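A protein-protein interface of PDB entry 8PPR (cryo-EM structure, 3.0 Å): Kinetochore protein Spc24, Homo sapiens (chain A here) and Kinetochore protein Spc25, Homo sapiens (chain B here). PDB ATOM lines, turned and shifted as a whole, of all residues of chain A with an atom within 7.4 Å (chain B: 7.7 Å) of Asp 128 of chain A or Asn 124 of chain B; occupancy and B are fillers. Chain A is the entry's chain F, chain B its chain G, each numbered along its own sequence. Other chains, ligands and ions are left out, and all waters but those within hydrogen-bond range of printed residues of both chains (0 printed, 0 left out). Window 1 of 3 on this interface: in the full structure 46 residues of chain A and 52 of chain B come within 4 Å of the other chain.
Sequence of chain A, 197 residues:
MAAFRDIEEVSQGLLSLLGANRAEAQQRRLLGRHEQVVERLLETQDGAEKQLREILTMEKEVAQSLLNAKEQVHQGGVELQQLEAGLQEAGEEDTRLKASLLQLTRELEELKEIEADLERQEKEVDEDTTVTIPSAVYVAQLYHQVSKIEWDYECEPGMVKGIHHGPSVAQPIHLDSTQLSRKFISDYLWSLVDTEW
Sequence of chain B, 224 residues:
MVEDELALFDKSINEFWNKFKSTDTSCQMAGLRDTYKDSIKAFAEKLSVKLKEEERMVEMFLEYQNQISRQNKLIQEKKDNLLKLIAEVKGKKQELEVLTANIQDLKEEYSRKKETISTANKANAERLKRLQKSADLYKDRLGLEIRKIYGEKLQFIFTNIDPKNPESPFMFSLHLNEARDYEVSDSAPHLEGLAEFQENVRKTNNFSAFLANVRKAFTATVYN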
ATOM      1  N   GLU A 122       1.256  10.194  14.495  1.00  0.00           N
ATOM      2  CA  GLU A 122       2.576   9.600  14.708  1.00  0.00           C
ATOM      3  C   GLU A 122       3.650  10.355  13.930  1.00  0.00           C
ATOM      4  O   GLU A 122       4.734  10.656  14.457  1.00  0.00           O
ATOM      5  CB  GLU A 122       2.559   8.125  14.305  1.00  0.00           C
ATOM      6  CG  GLU A 122       3.814   7.369  14.705  1.00  0.00           C
ATOM      7  CD  GLU A 122       4.835   7.288  13.584  1.00  0.00           C
ATOM      8  OE1 GLU A 122       4.542   7.765  12.467  1.00  0.00           O
ATOM      9  OE2 GLU A 122       5.937   6.755  13.827  1.00  0.00           O
ATOM     10  N   LYS A 123       3.359  10.677  12.668  1.00  0.00           N
ATOM     11  CA  LYS A 123       4.300  11.454  11.871  1.00  0.00           C
ATOM     12  C   LYS A 123       4.507  12.837  12.474  1.00  0.00           C
ATOM     13  O   LYS A 123       5.624  13.369  12.474  1.00  0.00           O
ATOM     14  CB  LYS A 123       3.810  11.561  10.427  1.00  0.00           C
ATOM     15  CG  LYS A 123       4.740  12.358   9.533  1.00  0.00           C
ATOM     16  CD  LYS A 123       6.057  11.632   9.335  1.00  0.00           C
ATOM     17  CE  LYS A 123       6.931  12.346   8.319  1.00  0.00           C
ATOM     18  NZ  LYS A 123       7.372  13.681   8.811  1.00  0.00           N
ATOM     19  N   GLU A 124       3.432  13.437  12.991  1.00  0.00           N
ATOM     20  CA  GLU A 124       3.551  14.735  13.645  1.00  0.00           C
ATOM     21  C   GLU A 124       4.457  14.648  14.868  1.00  0.00           C
ATOM     22  O   GLU A 124       5.270  15.544  15.113  1.00  0.00           O
ATOM     23  CB  GLU A 124       2.163  15.251  14.026  1.00  0.00           C
ATOM     24  CG  GLU A 124       2.115  16.727  14.389  1.00  0.00           C
ATOM     25  CD  GLU A 124       2.508  16.990  15.828  1.00  0.00           C
ATOM     26  OE1 GLU A 124       2.285  16.100  16.676  1.00  0.00           O
ATOM     27  OE2 GLU A 124       3.037  18.085  16.111  1.00  0.00           O
ATOM     28  N   VAL A 125       4.326  13.573  15.648  1.00  0.00           N
ATOM     29  CA  VAL A 125       5.185  13.382  16.816  1.00  0.00           C
ATOM     30  C   VAL A 125       6.642  13.321  16.392  1.00  0.00           C
ATOM     31  O   VAL A 125       7.510  13.985  16.976  1.00  0.00           O
ATOM     32  CB  VAL A 125       4.788  12.107  17.583  1.00  0.00           C
ATOM     33  CG1 VAL A 125       5.788  11.830  18.697  1.00  0.00           C
ATOM     34  CG2 VAL A 125       3.401  12.229  18.147  1.00  0.00           C
ATOM     35  N   ASP A 126       6.936  12.498  15.383  1.00  0.00           N
ATOM     36  CA  ASP A 126       8.319  12.358  14.940  1.00  0.00           C
ATOM     37  C   ASP A 126       8.874  13.690  14.451  1.00  0.00           C
ATOM     38  O   ASP A 126       9.961  14.115  14.866  1.00  0.00           O
ATOM     39  CB  ASP A 126       8.417  11.296  13.846  1.00  0.00           C
ATOM     40  CG  ASP A 126       8.148   9.903  14.368  1.00  0.00           C
ATOM     41  OD1 ASP A 126       8.422   9.654  15.561  1.00  0.00           O
ATOM     42  OD2 ASP A 126       7.661   9.057  13.588  1.00  0.00           O
ATOM     43  N   GLU A 127       8.126  14.373  13.581  1.00  0.00           N
ATOM     44  CA  GLU A 127       8.566  15.661  13.055  1.00  0.00           C
ATOM     45  C   GLU A 127       8.806  16.660  14.178  1.00  0.00           C
ATOM     46  O   GLU A 127       9.849  17.327  14.222  1.00  0.00           O
ATOM     47  CB  GLU A 127       7.528  16.195  12.066  1.00  0.00           C
ATOM     48  CG  GLU A 127       7.991  17.376  11.228  1.00  0.00           C
ATOM     49  CD  GLU A 127       7.789  18.704  11.932  1.00  0.00           C
ATOM     50  OE1 GLU A 127       6.908  18.782  12.814  1.00  0.00           O
ATOM     51  OE2 GLU A 127       8.505  19.672  11.599  1.00  0.00           O
ATOM     52  N   ASP A 128       7.847  16.770  15.102  1.00  0.00           N
ATOM     53  CA  ASP A 128       7.985  17.688  16.222  1.00  0.00           C
ATOM     54  C   ASP A 128       9.259  17.392  16.993  1.00  0.00           C
ATOM     55  O   ASP A 128      10.197  18.190  16.973  1.00  0.00           O
ATOM     56  CB  ASP A 128       6.758  17.594  17.131  1.00  0.00           C
ATOM     57  CG  ASP A 128       6.870  18.484  18.353  1.00  0.00           C
ATOM     58  OD1 ASP A 128       6.987  19.716  18.182  1.00  0.00           O
ATOM     59  OD2 ASP A 128       6.834  17.955  19.483  1.00  0.00           O
ATOM     60  N   THR A 129       9.351  16.194  17.575  1.00  0.00           N
ATOM     61  CA  THR A 129      10.494  15.806  18.395  1.00  0.00           C
ATOM     62  C   THR A 129      11.822  16.075  17.697  1.00  0.00           C
ATOM     63  O   THR A 129      12.729  16.677  18.288  1.00  0.00           O
ATOM     64  CB  THR A 129      10.400  14.326  18.770  1.00  0.00           C
ATOM     65  OG1 THR A 129       9.069  14.026  19.206  1.00  0.00           O
ATOM     66  CG2 THR A 129      11.384  13.992  19.880  1.00  0.00           C
ATOM     67  N   THR A 130      11.952  15.628  16.444  1.00  0.00           N
ATOM     68  CA  THR A 130      13.171  15.877  15.684  1.00  0.00           C
ATOM     69  C   THR A 130      13.478  17.366  15.571  1.00  0.00           C
ATOM     70  O   THR A 130      14.618  17.774  15.797  1.00  0.00           O
ATOM     71  CB  THR A 130      13.088  15.246  14.294  1.00  0.00           C
ATOM     72  OG1 THR A 130      11.963  15.777  13.584  1.00  0.00           O
ATOM     73  CG2 THR A 130      12.980  13.730  14.399  1.00  0.00           C
ATOM     74  N   VAL A 131      12.496  18.189  15.206  1.00  0.00           N
ATOM     75  CA  VAL A 131      12.747  19.625  15.128  1.00  0.00           C
ATOM     76  C   VAL A 131      13.173  20.159  16.491  1.00  0.00           C
ATOM     77  O   VAL A 131      14.271  20.703  16.639  1.00  0.00           O
ATOM     78  CB  VAL A 131      11.518  20.385  14.601  1.00  0.00           C
ATOM     79  CG1 VAL A 131      11.753  21.882  14.692  1.00  0.00           C
ATOM     80  CG2 VAL A 131      11.246  19.992  13.165  1.00  0.00           C
ATOM     81  N   THR A 132      12.309  19.988  17.489  1.00  0.00           N
ATOM     82  CA  THR A 132      12.505  20.515  18.834  1.00  0.00           C
ATOM     83  C   THR A 132      13.874  20.196  19.415  1.00  0.00           C
ATOM     84  O   THR A 132      14.641  21.113  19.726  1.00  0.00           O
ATOM     85  CB  THR A 132      11.429  19.980  19.784  1.00  0.00           C
ATOM     86  OG1 THR A 132      11.605  18.568  19.963  1.00  0.00           O
ATOM     87  CG2 THR A 132      10.039  20.267  19.245  1.00  0.00           C
ATOM     88  N   ILE A 133      14.193  18.914  19.569  1.00  0.00           N
ATOM     89  CA  ILE A 133      15.321  18.543  20.420  1.00  0.00           C
ATOM     90  C   ILE A 133      16.646  18.994  19.804  1.00  0.00           C
ATOM     91  O   ILE A 133      17.369  19.756  20.462  1.00  0.00           O
ATOM     92  CB  ILE A 133      15.294  17.042  20.760  1.00  0.00           C
ATOM     93  CG1 ILE A 133      13.922  16.657  21.315  1.00  0.00           C
ATOM     94  CG2 ILE A 133      16.402  16.699  21.741  1.00  0.00           C
ATOM     95  CD1 ILE A 133      13.504  17.478  22.516  1.00  0.00           C
ATOM     96  N   PRO A 134      17.042  18.563  18.570  1.00  0.00           N
ATOM     97  CA  PRO A 134      18.213  19.190  17.943  1.00  0.00           C
ATOM     98  C   PRO A 134      18.216  20.708  18.006  1.00  0.00           C
ATOM     99  O   PRO A 134      19.222  21.307  18.391  1.00  0.00           O
ATOM    100  CB  PRO A 134      18.123  18.705  16.493  1.00  0.00           C
ATOM    101  CG  PRO A 134      17.455  17.376  16.580  1.00  0.00           C
ATOM    102  CD  PRO A 134      16.826  17.240  17.955  1.00  0.00           C
ATOM    103  N   SER B 118      -0.215  10.234  22.163  1.00  0.00           N
ATOM    104  CA  SER B 118      -0.535  11.429  22.936  1.00  0.00           C
ATOM    105  C   SER B 118       0.462  11.642  24.071  1.00  0.00           C
ATOM    106  O   SER B 118       0.922  12.768  24.304  1.00  0.00           O
ATOM    107  CB  SER B 118      -1.961  11.327  23.480  1.00  0.00           C
ATOM    108  OG  SER B 118      -2.105  10.194  24.318  1.00  0.00           O
ATOM    109  N   THR B 119       0.807  10.574  24.793  1.00  0.00           N
ATOM    110  CA  THR B 119       1.735  10.744  25.909  1.00  0.00           C
ATOM    111  C   THR B 119       3.137  11.089  25.414  1.00  0.00           C
ATOM    112  O   THR B 119       3.863  11.854  26.065  1.00  0.00           O
ATOM    113  CB  THR B 119       1.748   9.501  26.806  1.00  0.00           C
ATOM    114  OG1 THR B 119       2.495   9.784  27.996  1.00  0.00           O
ATOM    115  CG2 THR B 119       2.366   8.307  26.106  1.00  0.00           C
ATOM    116  N   ALA B 120       3.533  10.552  24.254  1.00  0.00           N
ATOM    117  CA  ALA B 120       4.800  10.962  23.656  1.00  0.00           C
ATOM    118  C   ALA B 120       4.782  12.444  23.307  1.00  0.00           C
ATOM    119  O   ALA B 120       5.768  13.160  23.542  1.00  0.00           O
ATOM    120  CB  ALA B 120       5.093  10.119  22.415  1.00  0.00           C
ATOM    121  N   ASN B 121       3.667  12.920  22.743  1.00  0.00           N
ATOM    122  CA  ASN B 121       3.514  14.350  22.488  1.00  0.00           C
ATOM    123  C   ASN B 121       3.697  15.157  23.764  1.00  0.00           C
ATOM    124  O   ASN B 121       4.419  16.159  23.776  1.00  0.00           O
ATOM    125  CB  ASN B 121       2.143  14.641  21.878  1.00  0.00           C
ATOM    126  CG  ASN B 121       2.108  14.418  20.388  1.00  0.00           C
ATOM    127  OD1 ASN B 121       3.008  14.851  19.668  1.00  0.00           O
ATOM    128  ND2 ASN B 121       1.066  13.748  19.911  1.00  0.00           N
ATOM    129  N   LYS B 122       3.042  14.738  24.846  1.00  0.00           N
ATOM    130  CA  LYS B 122       3.120  15.498  26.091  1.00  0.00           C
ATOM    131  C   LYS B 122       4.547  15.539  26.629  1.00  0.00           C
ATOM    132  O   LYS B 122       5.034  16.596  27.051  1.00  0.00           O
ATOM    133  CB  LYS B 122       2.168  14.908  27.130  1.00  0.00           C
ATOM    134  CG  LYS B 122       0.728  14.820  26.663  1.00  0.00           C
ATOM    135  CD  LYS B 122      -0.179  14.315  27.766  1.00  0.00           C
ATOM    136  CE  LYS B 122      -1.547  13.942  27.222  1.00  0.00           C
ATOM    137  NZ  LYS B 122      -1.480  12.721  26.378  1.00  0.00           N
ATOM    138  N   ALA B 123       5.237  14.396  26.615  1.00  0.00           N
ATOM    139  CA  ALA B 123       6.602  14.354  27.131  1.00  0.00           C
ATOM    140  C   ALA B 123       7.530  15.241  26.308  1.00  0.00           C
ATOM    141  O   ALA B 123       8.300  16.043  26.860  1.00  0.00           O
ATOM    142  CB  ALA B 123       7.110  12.913  27.150  1.00  0.00           C
ATOM    143  N   ASN B 124       7.467  15.113  24.979  1.00  0.00           N
ATOM    144  CA  ASN B 124       8.324  15.930  24.127  1.00  0.00           C
ATOM    145  C   ASN B 124       7.998  17.408  24.285  1.00  0.00           C
ATOM    146  O   ASN B 124       8.900  18.254  24.279  1.00  0.00           O
ATOM    147  CB  ASN B 124       8.185  15.499  22.668  1.00  0.00           C
ATOM    148  CG  ASN B 124       9.048  16.324  21.735  1.00  0.00           C
ATOM    149  OD1 ASN B 124      10.274  16.326  21.845  1.00  0.00           O
ATOM    150  ND2 ASN B 124       8.412  17.030  20.809  1.00  0.00           N
ATOM    151  N   ALA B 125       6.714  17.739  24.435  1.00  0.00           N
ATOM    152  CA  ALA B 125       6.317  19.127  24.623  1.00  0.00           C
ATOM    153  C   ALA B 125       6.884  19.689  25.917  1.00  0.00           C
ATOM    154  O   ALA B 125       7.371  20.821  25.948  1.00  0.00           O
ATOM    155  CB  ALA B 125       4.792  19.243  24.605  1.00  0.00           C
ATOM    156  N   GLU B 126       6.822  18.916  27.004  1.00  0.00           N
ATOM    157  CA  GLU B 126       7.367  19.398  28.271  1.00  0.00           C
ATOM    158  C   GLU B 126       8.874  19.601  28.183  1.00  0.00           C
ATOM    159  O   GLU B 126       9.411  20.598  28.692  1.00  0.00           O
ATOM    160  CB  GLU B 126       7.020  18.427  29.397  1.00  0.00           C
ATOM    161  CG  GLU B 126       5.535  18.337  29.678  1.00  0.00           C
ATOM    162  CD  GLU B 126       4.962  19.653  30.163  1.00  0.00           C
ATOM    163  OE1 GLU B 126       5.689  20.407  30.843  1.00  0.00           O
ATOM    164  OE2 GLU B 126       3.785  19.938  29.858  1.00  0.00           O
ATOM    165  N   ARG B 127       9.576  18.665  27.540  1.00  0.00           N
ATOM    166  CA  ARG B 127      11.015  18.829  27.358  1.00  0.00           C
ATOM    167  C   ARG B 127      11.319  20.081  26.541  1.00  0.00           C
ATOM    168  O   ARG B 127      12.230  20.853  26.873  1.00  0.00           O
ATOM    169  CB  ARG B 127      11.594  17.581  26.693  1.00  0.00           C
ATOM    170  CG  ARG B 127      11.436  16.328  27.537  1.00  0.00           C
ATOM    171  CD  ARG B 127      11.745  15.070  26.750  1.00  0.00           C
ATOM    172  NE  ARG B 127      13.104  15.070  26.223  1.00  0.00           N
ATOM    173  CZ  ARG B 127      13.405  14.947  24.938  1.00  0.00           C
ATOM    174  NH1 ARG B 127      12.463  14.788  24.021  1.00  0.00           N
ATOM    175  NH2 ARG B 127      14.680  14.980  24.564  1.00  0.00           N
ATOM    176  N   LEU B 128      10.545  20.307  25.478  1.00  0.00           N
ATOM    177  CA  LEU B 128      10.732  21.501  24.663  1.00  0.00           C
ATOM    178  C   LEU B 128      10.440  22.767  25.455  1.00  0.00           C
ATOM    179  O   LEU B 128      11.102  23.788  25.263  1.00  0.00           O
ATOM    180  CB  LEU B 128       9.850  21.432  23.418  1.00  0.00           C
ATOM    181  CG  LEU B 128       9.774  22.720  22.596  1.00  0.00           C
ATOM    182  CD1 LEU B 128      11.084  22.971  21.865  1.00  0.00           C
ATOM    183  CD2 LEU B 128       8.610  22.670  21.621  1.00  0.00           C
ATOM    184  N   LYS B 129       9.440  22.728  26.336  1.00  0.00           N
ATOM    185  CA  LYS B 129       9.135  23.892  27.164  1.00  0.00           C
ATOM    186  C   LYS B 129      10.289  24.214  28.100  1.00  0.00           C
ATOM    187  O   LYS B 129      10.649  25.382  28.282  1.00  0.00           O
ATOM    188  CB  LYS B 129       7.851  23.658  27.960  1.00  0.00           C
ATOM    189  CG  LYS B 129       6.614  23.495  27.106  1.00  0.00           C
ATOM    190  CD  LYS B 129       5.453  22.959  27.918  1.00  0.00           C
ATOM    191  CE  LYS B 129       4.269  22.633  27.026  1.00  0.00           C
ATOM    192  NZ  LYS B 129       3.813  23.826  26.262  1.00  0.00           N
ATOM    193  N   ARG B 130      10.879  23.186  28.713  1.00  0.00           N
ATOM    194  CA  ARG B 130      12.043  23.421  29.564  1.00  0.00           C
ATOM    195  C   ARG B 130      13.194  24.021  28.761  1.00  0.00           C
ATOM    196  O   ARG B 130      13.831  24.997  29.189  1.00  0.00           O
ATOM    197  CB  ARG B 130      12.478  22.115  30.225  1.00  0.00           C
ATOM    198  CG  ARG B 130      11.624  21.694  31.405  1.00  0.00           C
ATOM    199  CD  ARG B 130      12.352  20.673  32.259  1.00  0.00           C
ATOM    200  NE  ARG B 130      11.559  20.247  33.405  1.00  0.00           N
ATOM    201  CZ  ARG B 130      11.174  18.997  33.623  1.00  0.00           C
ATOM    202  NH1 ARG B 130      11.494  18.021  32.789  1.00  0.00           N
ATOM    203  NH2 ARG B 130      10.454  18.719  34.706  1.00  0.00           N
ATOM    204  N   LEU B 131      13.458  23.455  27.581  1.00  0.00           N
ATOM    205  CA  LEU B 131      14.535  23.963  26.738  1.00  0.00           C
ATOM    206  C   LEU B 131      14.268  25.399  26.305  1.00  0.00           C
ATOM    207  O   LEU B 131      15.187  26.225  26.262  1.00  0.00           O
ATOM    208  CB  LEU B 131      14.705  23.056  25.523  1.00  0.00           C
ATOM    209  CG  LEU B 131      15.184  21.634  25.816  1.00  0.00           C
ATOM    210  CD1 LEU B 131      15.073  20.767  24.574  1.00  0.00           C
ATOM    211  CD2 LEU B 131      16.611  21.644  26.337  1.00  0.00           C
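Printed residues of chain B within 4 Å of Asp 128 of chain A: Asn 124 (2.3 Å). Of chain A, only Asp 128, Thr 129, Thr 132 and Ile 133 come within 4 Å of Asn 124 of chain B. No residue of chain A comes within 4 Å of Ala 123 of chain B. Of the printed residues of chain A, Arg 127 of chain B touches Ile 133 (3.3 Å). Printed residues of chain A within 4 Å of Leu 128 of chain B: Thr 132. Printed residues of chain B within 4 Å of Thr 129 of chain A: Asn 124. The nearest residue of chain A that does not touch Asn 124 of chain B is Val 125 of chain A (5.0 Å). The nearest printed residue of chain A that does not touch Asn 121 of chain B is Asp 128 of chain A (4.9 Å).
Of the 13 printed residues of chain A, 6 touch a printed residue of chain B. Hydrophobic or aromatic side chains of chain B that line the printed part of chain A: Leu 128. Among the printed residues, 8 pairs touch across the chains. Among the printed residues, no Asp or Glu carboxylate lies within 4 Å of a Lys or Arg side-chain nitrogen of the other chain.
Val 125 of chain A touches Asn 121 of chain B (CG2 to OD1, 3.1 Å). Thr 132 of chain A touches Leu 128 of chain B. Asn 124 of chain B touches Ile 133 of chain A. Ile 133 of chain A touches Arg 127 of chain B.
OE1 of Glu 124 of chain A sits close to OD1 of Asn 121 of chain B (3.3 Å). The side-chain amide nitrogen (ND2) of Asn 124 of chain B sits close to the side-chain hydroxyl (OG1) of Thr 129 of chain A (3.5 Å). The side-chain hydroxyl (OG1) of Thr 132 of chain A lies within hydrogen-bond range of the side-chain amide oxygen (OD1) of Asn 124 of chain B (3.2 Å). ND2 of Asn 124 of chain B sits close to OD2 of Asp 128 of chain A (2.3 Å).
O of Val 125 of chain A sits at hydrogen-bond distance from OG1 of Thr 129 of chain A (2.7 Å). O of Asp 128 of chain A sits close to OG1 of Thr 132 of chain A. The backbone carbonyl oxygen (O) of Thr 129 of chain A sits at hydrogen-bond distance from the side-chain hydroxyl (OG1) of Thr 132 of chain A, at 2.8 Å. The side-chain amide oxygen of Asn 124 of chain B is in hydrogen-bond range of the guanidinium group of Arg 127 of chain B, at 3.4 Å.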
